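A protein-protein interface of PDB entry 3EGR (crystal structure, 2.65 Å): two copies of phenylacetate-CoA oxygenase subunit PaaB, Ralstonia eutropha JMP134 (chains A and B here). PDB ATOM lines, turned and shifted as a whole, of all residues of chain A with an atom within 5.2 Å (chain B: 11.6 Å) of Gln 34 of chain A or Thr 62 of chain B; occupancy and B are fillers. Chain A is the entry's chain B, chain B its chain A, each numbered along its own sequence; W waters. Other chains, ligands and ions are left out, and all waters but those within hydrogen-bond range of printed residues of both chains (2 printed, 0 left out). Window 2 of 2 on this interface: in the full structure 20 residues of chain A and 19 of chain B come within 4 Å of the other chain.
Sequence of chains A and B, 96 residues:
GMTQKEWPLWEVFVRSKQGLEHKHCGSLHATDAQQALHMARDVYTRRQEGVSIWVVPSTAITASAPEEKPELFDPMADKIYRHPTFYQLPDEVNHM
Along chain B the printed residues that touch a printed residue of chain A span positions 13 to 64. Hydrophobic or aromatic side chains of chain A within 4 Å of the printed part of chain B: Ala 33, Leu 37, Trp 54 and Val 55.
Water W2 lies within hydrogen-bond range of OG1 of Thr 62 of chain B (2.6 Å), O of Ala 60 of chain B (2.7 Å) and O of Val 55 of chain A (3.3 Å). Water W1 lies within hydrogen-bond range of the side-chain amide nitrogen of Gln 34 of chain A and the backbone carbonyl oxygen of Ala 63 of chain B.
The backbone NH (N) of Ser 64 of chain B is in hydrogen-bond range of the backbone carbonyl oxygen (O) of Ile 53 of chain A (2.9 Å). The backbone carbonyl oxygen (O) of Thr 62 of chain B is in hydrogen-bond range of the backbone NH (N) of Val 55 of chain A (3.0 Å).
Of the printed residues of chain B, Gln 34 of chain A touches Thr 62 (3.7 Å). Thr 62 of chain B touches just these residues of chain A: Ala 33 (3.4 Å), Gln 34 (3.7 Å), Leu 37 (3.9 Å), Ile 53 (3.9 Å), Trp 54 (3.5 Å) and Val 55 (3.0 Å). No residue of chain B comes within 4 Å of Asp 32 of chain A. Of chain B, only Thr 62 comes within 4 Å of Ala 33 of chain A. No residue of chain B comes within 4 Å of Gln 35 of chain A. Of the printed residues of chain A, Phe 13 of chain B touches Trp 54 (3.8 Å). Of the printed residues of chain A, Ala 63 of chain B touches Leu 37 (3.6 Å), Ile 53 (3.4 Å) and Trp 54 (3.6 Å). Glu 11 of chain B touches none of the printed residues of chain A. Met 39 of chain A touches none of the printed residues of chain B. The nearest residue of chain B that does not touch Gln 34 of chain A is Ala 63 of chain B (5.3 Å).
No position is printed for both chains. Of the 14 pairs that touch across the chains among the printed residues, none has its exchanged pair printed and touching as well.
Among the printed residues, merely in contact across the chains: Ile 53 of chain A with Ala 63 of chain B, Ala 33 of chain A with Thr 62 of chain B, Val 55 of chain A with Ile 61 of chain B, Trp 54 of chain A with Thr 62 of chain B, Val 55 of chain A with Ala 60 of chain B, Trp 54 of chain A with Ala 63 of chain B, Trp 54 of chain A with Ile 61 of chain B, Leu 37 of chain A with Ala 63 of chain B, Gln 34 of chain A with Thr 62 of chain B, Trp 54 of chain A with Phe 13 of chain B, Ile 53 of chain A with Thr 62 of chain B and Leu 37 of chain A with Thr 62 of chain B.
The backbone carbonyl oxygen of Gln 34 of chain A sits at hydrogen-bond distance from a ring nitrogen (ND1) of His 38 of chain A, 3.2 Å away. OD1 of Asp 32 of chain A lies within hydrogen-bond range of N of Gln 34 of chain A, 3.0 Å away.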
ATOM      1  N   ASP A  32      28.419  -7.219   1.590  1.00  0.00           N
ATOM      2  CA  ASP A  32      27.210  -6.405   1.493  1.00  0.00           C
ATOM      3  C   ASP A  32      26.066  -7.018   2.283  1.00  0.00           C
ATOM      4  O   ASP A  32      26.220  -8.101   2.851  1.00  0.00           O
ATOM      5  CB  ASP A  32      26.834  -6.207   0.027  1.00  0.00           C
ATOM      6  CG  ASP A  32      26.487  -7.488  -0.677  1.00  0.00           C
ATOM      7  OD1 ASP A  32      25.858  -8.390  -0.093  1.00  0.00           O
ATOM      8  OD2 ASP A  32      26.820  -7.584  -1.857  1.00  0.00           O
ATOM      9  N   ALA A  33      24.929  -6.327   2.313  1.00  0.00           N
ATOM     10  CA  ALA A  33      23.778  -6.768   3.110  1.00  0.00           C
ATOM     11  C   ALA A  33      23.235  -8.120   2.639  1.00  0.00           C
ATOM     12  O   ALA A  33      22.845  -8.959   3.454  1.00  0.00           O
ATOM     13  CB  ALA A  33      22.652  -5.681   3.130  1.00  0.00           C
ATOM     14  N   GLN A  34      23.225  -8.343   1.335  1.00  0.00           N
ATOM     15  CA  GLN A  34      22.683  -9.588   0.795  1.00  0.00           C
ATOM     16  C   GLN A  34      23.567 -10.780   1.143  1.00  0.00           C
ATOM     17  O   GLN A  34      23.067 -11.857   1.522  1.00  0.00           O
ATOM     18  CB  GLN A  34      22.464  -9.463  -0.701  1.00  0.00           C
ATOM     19  CG  GLN A  34      21.362  -8.447  -1.042  1.00  0.00           C
ATOM     20  CD  GLN A  34      19.994  -8.785  -0.390  1.00  0.00           C
ATOM     21  OE1 GLN A  34      19.507  -9.925  -0.475  1.00  0.00           O
ATOM     22  NE2 GLN A  34      19.378  -7.793   0.251  1.00  0.00           N
ATOM     23  N   GLN A  35      24.877 -10.587   1.062  1.00  0.00           N
ATOM     24  CA  GLN A  35      25.795 -11.653   1.434  1.00  0.00           C
ATOM     25  C   GLN A  35      25.623 -11.921   2.921  1.00  0.00           C
ATOM     26  O   GLN A  35      25.559 -13.067   3.343  1.00  0.00           O
ATOM     27  CB  GLN A  35      27.250 -11.312   1.089  1.00  0.00           C
ATOM     28  CG  GLN A  35      28.179 -12.518   1.230  1.00  0.00           C
ATOM     29  CD  GLN A  35      29.686 -12.195   1.105  1.00  0.00           C
ATOM     30  OE1 GLN A  35      30.243 -11.352   1.830  1.00  0.00           O
ATOM     31  NE2 GLN A  35      30.354 -12.908   0.198  1.00  0.00           N
ATOM     32  N   ALA A  36      25.507 -10.865   3.717  1.00  0.00           N
ATOM     33  CA  ALA A  36      25.278 -11.047   5.136  1.00  0.00           C
ATOM     34  C   ALA A  36      23.994 -11.873   5.391  1.00  0.00           C
ATOM     35  O   ALA A  36      23.966 -12.719   6.280  1.00  0.00           O
ATOM     36  CB  ALA A  36      25.231  -9.716   5.850  1.00  0.00           C
ATOM     37  N   LEU A  37      22.940 -11.658   4.611  1.00  0.00           N
ATOM     38  CA  LEU A  37      21.715 -12.418   4.837  1.00  0.00           C
ATOM     39  C   LEU A  37      21.915 -13.906   4.507  1.00  0.00           C
ATOM     40  O   LEU A  37      21.551 -14.760   5.304  1.00  0.00           O
ATOM     41  CB  LEU A  37      20.540 -11.799   4.076  1.00  0.00           C
ATOM     42  CG  LEU A  37      19.937 -10.531   4.718  1.00  0.00           C
ATOM     43  CD1 LEU A  37      19.034  -9.752   3.749  1.00  0.00           C
ATOM     44  CD2 LEU A  37      19.178 -10.879   6.003  1.00  0.00           C
ATOM     45  N   HIS A  38      22.531 -14.214   3.370  1.00  0.00           N
ATOM     46  CA  HIS A  38      22.745 -15.617   2.994  1.00  0.00           C
ATOM     47  C   HIS A  38      23.663 -16.359   3.984  1.00  0.00           C
ATOM     48  O   HIS A  38      23.466 -17.546   4.239  1.00  0.00           O
ATOM     49  CB  HIS A  38      23.257 -15.732   1.552  1.00  0.00           C
ATOM     50  CG  HIS A  38      22.245 -15.328   0.522  1.00  0.00           C
ATOM     51  ND1 HIS A  38      22.464 -14.308  -0.382  1.00  0.00           N
ATOM     52  CD2 HIS A  38      20.997 -15.789   0.270  1.00  0.00           C
ATOM     53  CE1 HIS A  38      21.402 -14.168  -1.152  1.00  0.00           C
ATOM     54  NE2 HIS A  38      20.497 -15.054  -0.776  1.00  0.00           N
ATOM     55  N   MET A  39      24.659 -15.675   4.542  1.00  0.00           N
ATOM     56  CA  MET A  39      25.472 -16.266   5.610  1.00  0.00           C
ATOM     57  C   MET A  39      24.665 -16.508   6.883  1.00  0.00           C
ATOM     58  O   MET A  39      24.657 -17.619   7.432  1.00  0.00           O
ATOM     59  CB  MET A  39      26.623 -15.368   5.980  1.00  0.00           C
ATOM     60  CG  MET A  39      27.757 -15.368   5.010  1.00  0.00           C
ATOM     61  SD  MET A  39      29.354 -14.694   5.906  1.00  0.00           S
ATOM     62  CE  MET A  39      29.551 -16.037   7.285  1.00  0.00           C
ATOM     63  N   ILE A  53      15.283 -12.736   9.185  1.00  0.00           N
ATOM     64  CA  ILE A  53      16.630 -12.293   9.530  1.00  0.00           C
ATOM     65  C   ILE A  53      16.780 -10.809   9.220  1.00  0.00           C
ATOM     66  O   ILE A  53      16.375 -10.339   8.142  1.00  0.00           O
ATOM     67  CB  ILE A  53      17.702 -13.087   8.746  1.00  0.00           C
ATOM     68  CG1 ILE A  53      17.448 -14.601   8.909  1.00  0.00           C
ATOM     69  CG2 ILE A  53      19.113 -12.687   9.221  1.00  0.00           C
ATOM     70  CD1 ILE A  53      18.412 -15.495   8.149  1.00  0.00           C
ATOM     71  N   TRP A  54      17.331 -10.068  10.175  1.00  0.00           N
ATOM     72  CA  TRP A  54      17.737  -8.694   9.931  1.00  0.00           C
ATOM     73  C   TRP A  54      19.267  -8.589  10.017  1.00  0.00           C
ATOM     74  O   TRP A  54      19.867  -9.127  10.951  1.00  0.00           O
ATOM     75  CB  TRP A  54      17.150  -7.750  10.987  1.00  0.00           C
ATOM     76  CG  TRP A  54      15.686  -7.496  10.936  1.00  0.00           C
ATOM     77  CD1 TRP A  54      14.813  -7.895   9.981  1.00  0.00           C
ATOM     78  CD2 TRP A  54      14.935  -6.728  11.876  1.00  0.00           C
ATOM     79  NE1 TRP A  54      13.550  -7.433  10.272  1.00  0.00           N
ATOM     80  CE2 TRP A  54      13.602  -6.710  11.431  1.00  0.00           C
ATOM     81  CE3 TRP A  54      15.265  -6.045  13.051  1.00  0.00           C
ATOM     82  CZ2 TRP A  54      12.597  -6.044  12.114  1.00  0.00           C
ATOM     83  CZ3 TRP A  54      14.274  -5.382  13.727  1.00  0.00           C
ATOM     84  CH2 TRP A  54      12.949  -5.380  13.252  1.00  0.00           C
ATOM     85  N   VAL A  55      19.874  -7.871   9.067  1.00  0.00           N
ATOM     86  CA  VAL A  55      21.270  -7.485   9.163  1.00  0.00           C
ATOM     87  C   VAL A  55      21.427  -5.959   9.255  1.00  0.00           C
ATOM     88  O   VAL A  55      20.684  -5.198   8.616  1.00  0.00           O
ATOM     89  CB  VAL A  55      22.114  -8.050   7.995  1.00  0.00           C
ATOM     90  CG1 VAL A  55      22.034  -9.537   8.003  1.00  0.00           C
ATOM     91  CG2 VAL A  55      21.677  -7.482   6.611  1.00  0.00           C
ATOM     92  N   GLU B  11      14.875   1.755  15.290  1.00  0.00           N
ATOM     93  CA  GLU B  11      14.523   0.514  15.951  1.00  0.00           C
ATOM     94  C   GLU B  11      15.316   0.419  17.249  1.00  0.00           C
ATOM     95  O   GLU B  11      16.492   0.816  17.310  1.00  0.00           O
ATOM     96  CB  GLU B  11      14.802  -0.690  15.056  1.00  0.00           C
ATOM     97  CG  GLU B  11      14.038  -0.688  13.733  1.00  0.00           C
ATOM     98  CD  GLU B  11      12.547  -0.571  13.905  1.00  0.00           C
ATOM     99  OE1 GLU B  11      11.997  -1.046  14.925  1.00  0.00           O
ATOM    100  OE2 GLU B  11      11.909  -0.011  13.001  1.00  0.00           O
ATOM    101  N   PHE B  13      16.580  -1.965  20.494  1.00  0.00           N
ATOM    102  CA  PHE B  13      16.875  -3.301  21.004  1.00  0.00           C
ATOM    103  C   PHE B  13      17.402  -3.142  22.413  1.00  0.00           C
ATOM    104  O   PHE B  13      18.257  -2.286  22.646  1.00  0.00           O
ATOM    105  CB  PHE B  13      17.941  -3.993  20.146  1.00  0.00           C
ATOM    106  CG  PHE B  13      17.620  -4.021  18.674  1.00  0.00           C
ATOM    107  CD1 PHE B  13      17.856  -2.915  17.877  1.00  0.00           C
ATOM    108  CD2 PHE B  13      17.090  -5.151  18.085  1.00  0.00           C
ATOM    109  CE1 PHE B  13      17.562  -2.935  16.530  1.00  0.00           C
ATOM    110  CE2 PHE B  13      16.792  -5.170  16.735  1.00  0.00           C
ATOM    111  CZ  PHE B  13      17.026  -4.060  15.964  1.00  0.00           C
ATOM    112  N   VAL B  56      19.016   1.990  16.326  1.00  0.00           N
ATOM    113  CA  VAL B  56      19.443   1.851  14.939  1.00  0.00           C
ATOM    114  C   VAL B  56      18.422   2.547  14.055  1.00  0.00           C
ATOM    115  O   VAL B  56      17.214   2.281  14.171  1.00  0.00           O
ATOM    116  CB  VAL B  56      19.482   0.375  14.517  1.00  0.00           C
ATOM    117  CG1 VAL B  56      20.134   0.242  13.184  1.00  0.00           C
ATOM    118  CG2 VAL B  56      20.205  -0.441  15.568  1.00  0.00           C
ATOM    119  N   PRO B  57      18.885   3.454  13.179  1.00  0.00           N
ATOM    120  CA  PRO B  57      17.942   4.011  12.233  1.00  0.00           C
ATOM    121  C   PRO B  57      17.404   2.890  11.363  1.00  0.00           C
ATOM    122  O   PRO B  57      18.184   2.034  10.930  1.00  0.00           O
ATOM    123  CB  PRO B  57      18.788   4.992  11.407  1.00  0.00           C
ATOM    124  CG  PRO B  57      20.173   4.724  11.725  1.00  0.00           C
ATOM    125  CD  PRO B  57      20.240   4.003  13.014  1.00  0.00           C
ATOM    126  N   SER B  58      16.087   2.894  11.150  1.00  0.00           N
ATOM    127  CA  SER B  58      15.399   1.915  10.310  1.00  0.00           C
ATOM    128  C   SER B  58      16.085   1.664   8.968  1.00  0.00           C
ATOM    129  O   SER B  58      16.219   0.522   8.531  1.00  0.00           O
ATOM    130  CB  SER B  58      13.961   2.375  10.048  1.00  0.00           C
ATOM    131  OG  SER B  58      13.133   2.171  11.180  1.00  0.00           O
ATOM    132  N   THR B  59      16.536   2.733   8.323  1.00  0.00           N
ATOM    133  CA  THR B  59      17.155   2.623   7.023  1.00  0.00           C
ATOM    134  C   THR B  59      18.386   1.741   7.043  1.00  0.00           C
ATOM    135  O   THR B  59      18.820   1.288   6.016  1.00  0.00           O
ATOM    136  CB  THR B  59      17.476   4.010   6.446  1.00  0.00           C
ATOM    137  OG1 THR B  59      18.207   4.795   7.411  1.00  0.00           O
ATOM    138  CG2 THR B  59      16.165   4.703   6.074  1.00  0.00           C
ATOM    139  N   ALA B  60      18.951   1.473   8.210  1.00  0.00           N
ATOM    140  CA  ALA B  60      20.166   0.666   8.306  1.00  0.00           C
ATOM    141  C   ALA B  60      19.880  -0.848   8.312  1.00  0.00           C
ATOM    142  O   ALA B  60      20.802  -1.644   8.195  1.00  0.00           O
ATOM    143  CB  ALA B  60      20.956   1.071   9.546  1.00  0.00           C
ATOM    144  N   ILE B  61      18.620  -1.242   8.451  1.00  0.00           N
ATOM    145  CA  ILE B  61      18.254  -2.655   8.552  1.00  0.00           C
ATOM    146  C   ILE B  61      17.843  -3.193   7.190  1.00  0.00           C
ATOM    147  O   ILE B  61      16.992  -2.616   6.549  1.00  0.00           O
ATOM    148  CB  ILE B  61      17.058  -2.851   9.550  1.00  0.00           C
ATOM    149  CG1 ILE B  61      17.486  -2.479  10.973  1.00  0.00           C
ATOM    150  CG2 ILE B  61      16.585  -4.270   9.542  1.00  0.00           C
ATOM    151  CD1 ILE B  61      16.357  -2.060  11.861  1.00  0.00           C
ATOM    152  N   THR B  62      18.445  -4.286   6.758  1.00  0.00           N
ATOM    153  CA  THR B  62      17.993  -5.028   5.587  1.00  0.00           C
ATOM    154  C   THR B  62      17.386  -6.345   6.093  1.00  0.00           C
ATOM    155  O   THR B  62      18.058  -7.116   6.800  1.00  0.00           O
ATOM    156  CB  THR B  62      19.175  -5.345   4.673  1.00  0.00           C
ATOM    157  OG1 THR B  62      19.947  -4.155   4.479  1.00  0.00           O
ATOM    158  CG2 THR B  62      18.721  -5.884   3.338  1.00  0.00           C
ATOM    159  N   ALA B  63      16.113  -6.580   5.757  1.00  0.00           N
ATOM    160  CA  ALA B  63      15.387  -7.791   6.162  1.00  0.00           C
ATOM    161  C   ALA B  63      15.428  -8.835   5.062  1.00  0.00           C
ATOM    162  O   ALA B  63      15.622  -8.517   3.893  1.00  0.00           O
ATOM    163  CB  ALA B  63      13.975  -7.468   6.499  1.00  0.00           C
ATOM    164  N   SER B  64      15.287 -10.092   5.445  1.00  0.00           N
ATOM    165  CA  SER B  64      15.147 -11.156   4.476  1.00  0.00           C
ATOM    166  C   SER B  64      13.755 -11.051   3.822  1.00  0.00           C
ATOM    167  O   SER B  64      12.808 -10.518   4.425  1.00  0.00           O
ATOM    168  CB  SER B  64      15.312 -12.496   5.160  1.00  0.00           C
ATOM    169  OG  SER B  64      14.472 -12.547   6.299  1.00  0.00           O
ATOM    170  N   ALA B  65      13.655 -11.569   2.594  1.00  0.00           N
ATOM    171  CA  ALA B  65      12.456 -11.466   1.763  1.00  0.00           C
ATOM    172  C   ALA B  65      11.453 -12.588   2.064  1.00  0.00           C
ATOM    173  O   ALA B  65      11.794 -13.771   1.925  1.00  0.00           O
ATOM    174  CB  ALA B  65      12.857 -11.526   0.304  1.00  0.00           C
ATOM    175  N   PRO B  66      10.214 -12.234   2.487  1.00  0.00           N
ATOM    176  CA  PRO B  66       9.119 -13.229   2.630  1.00  0.00           C
ATOM    177  C   PRO B  66       8.892 -14.098   1.395  1.00  0.00           C
ATOM    178  O   PRO B  66       9.298 -15.258   1.392  1.00  0.00           O
ATOM    179  CB  PRO B  66       7.883 -12.360   2.896  1.00  0.00           C
ATOM    180  CG  PRO B  66       8.435 -11.104   3.551  1.00  0.00           C
ATOM    181  CD  PRO B  66       9.791 -10.882   2.909  1.00  0.00           C
HETATM  182  O   HOH W   1      16.885  -8.403   1.372  1.00  0.00           O
HETATM  183  O   HOH W   2      21.647  -3.195   6.127  1.00  0.00           O
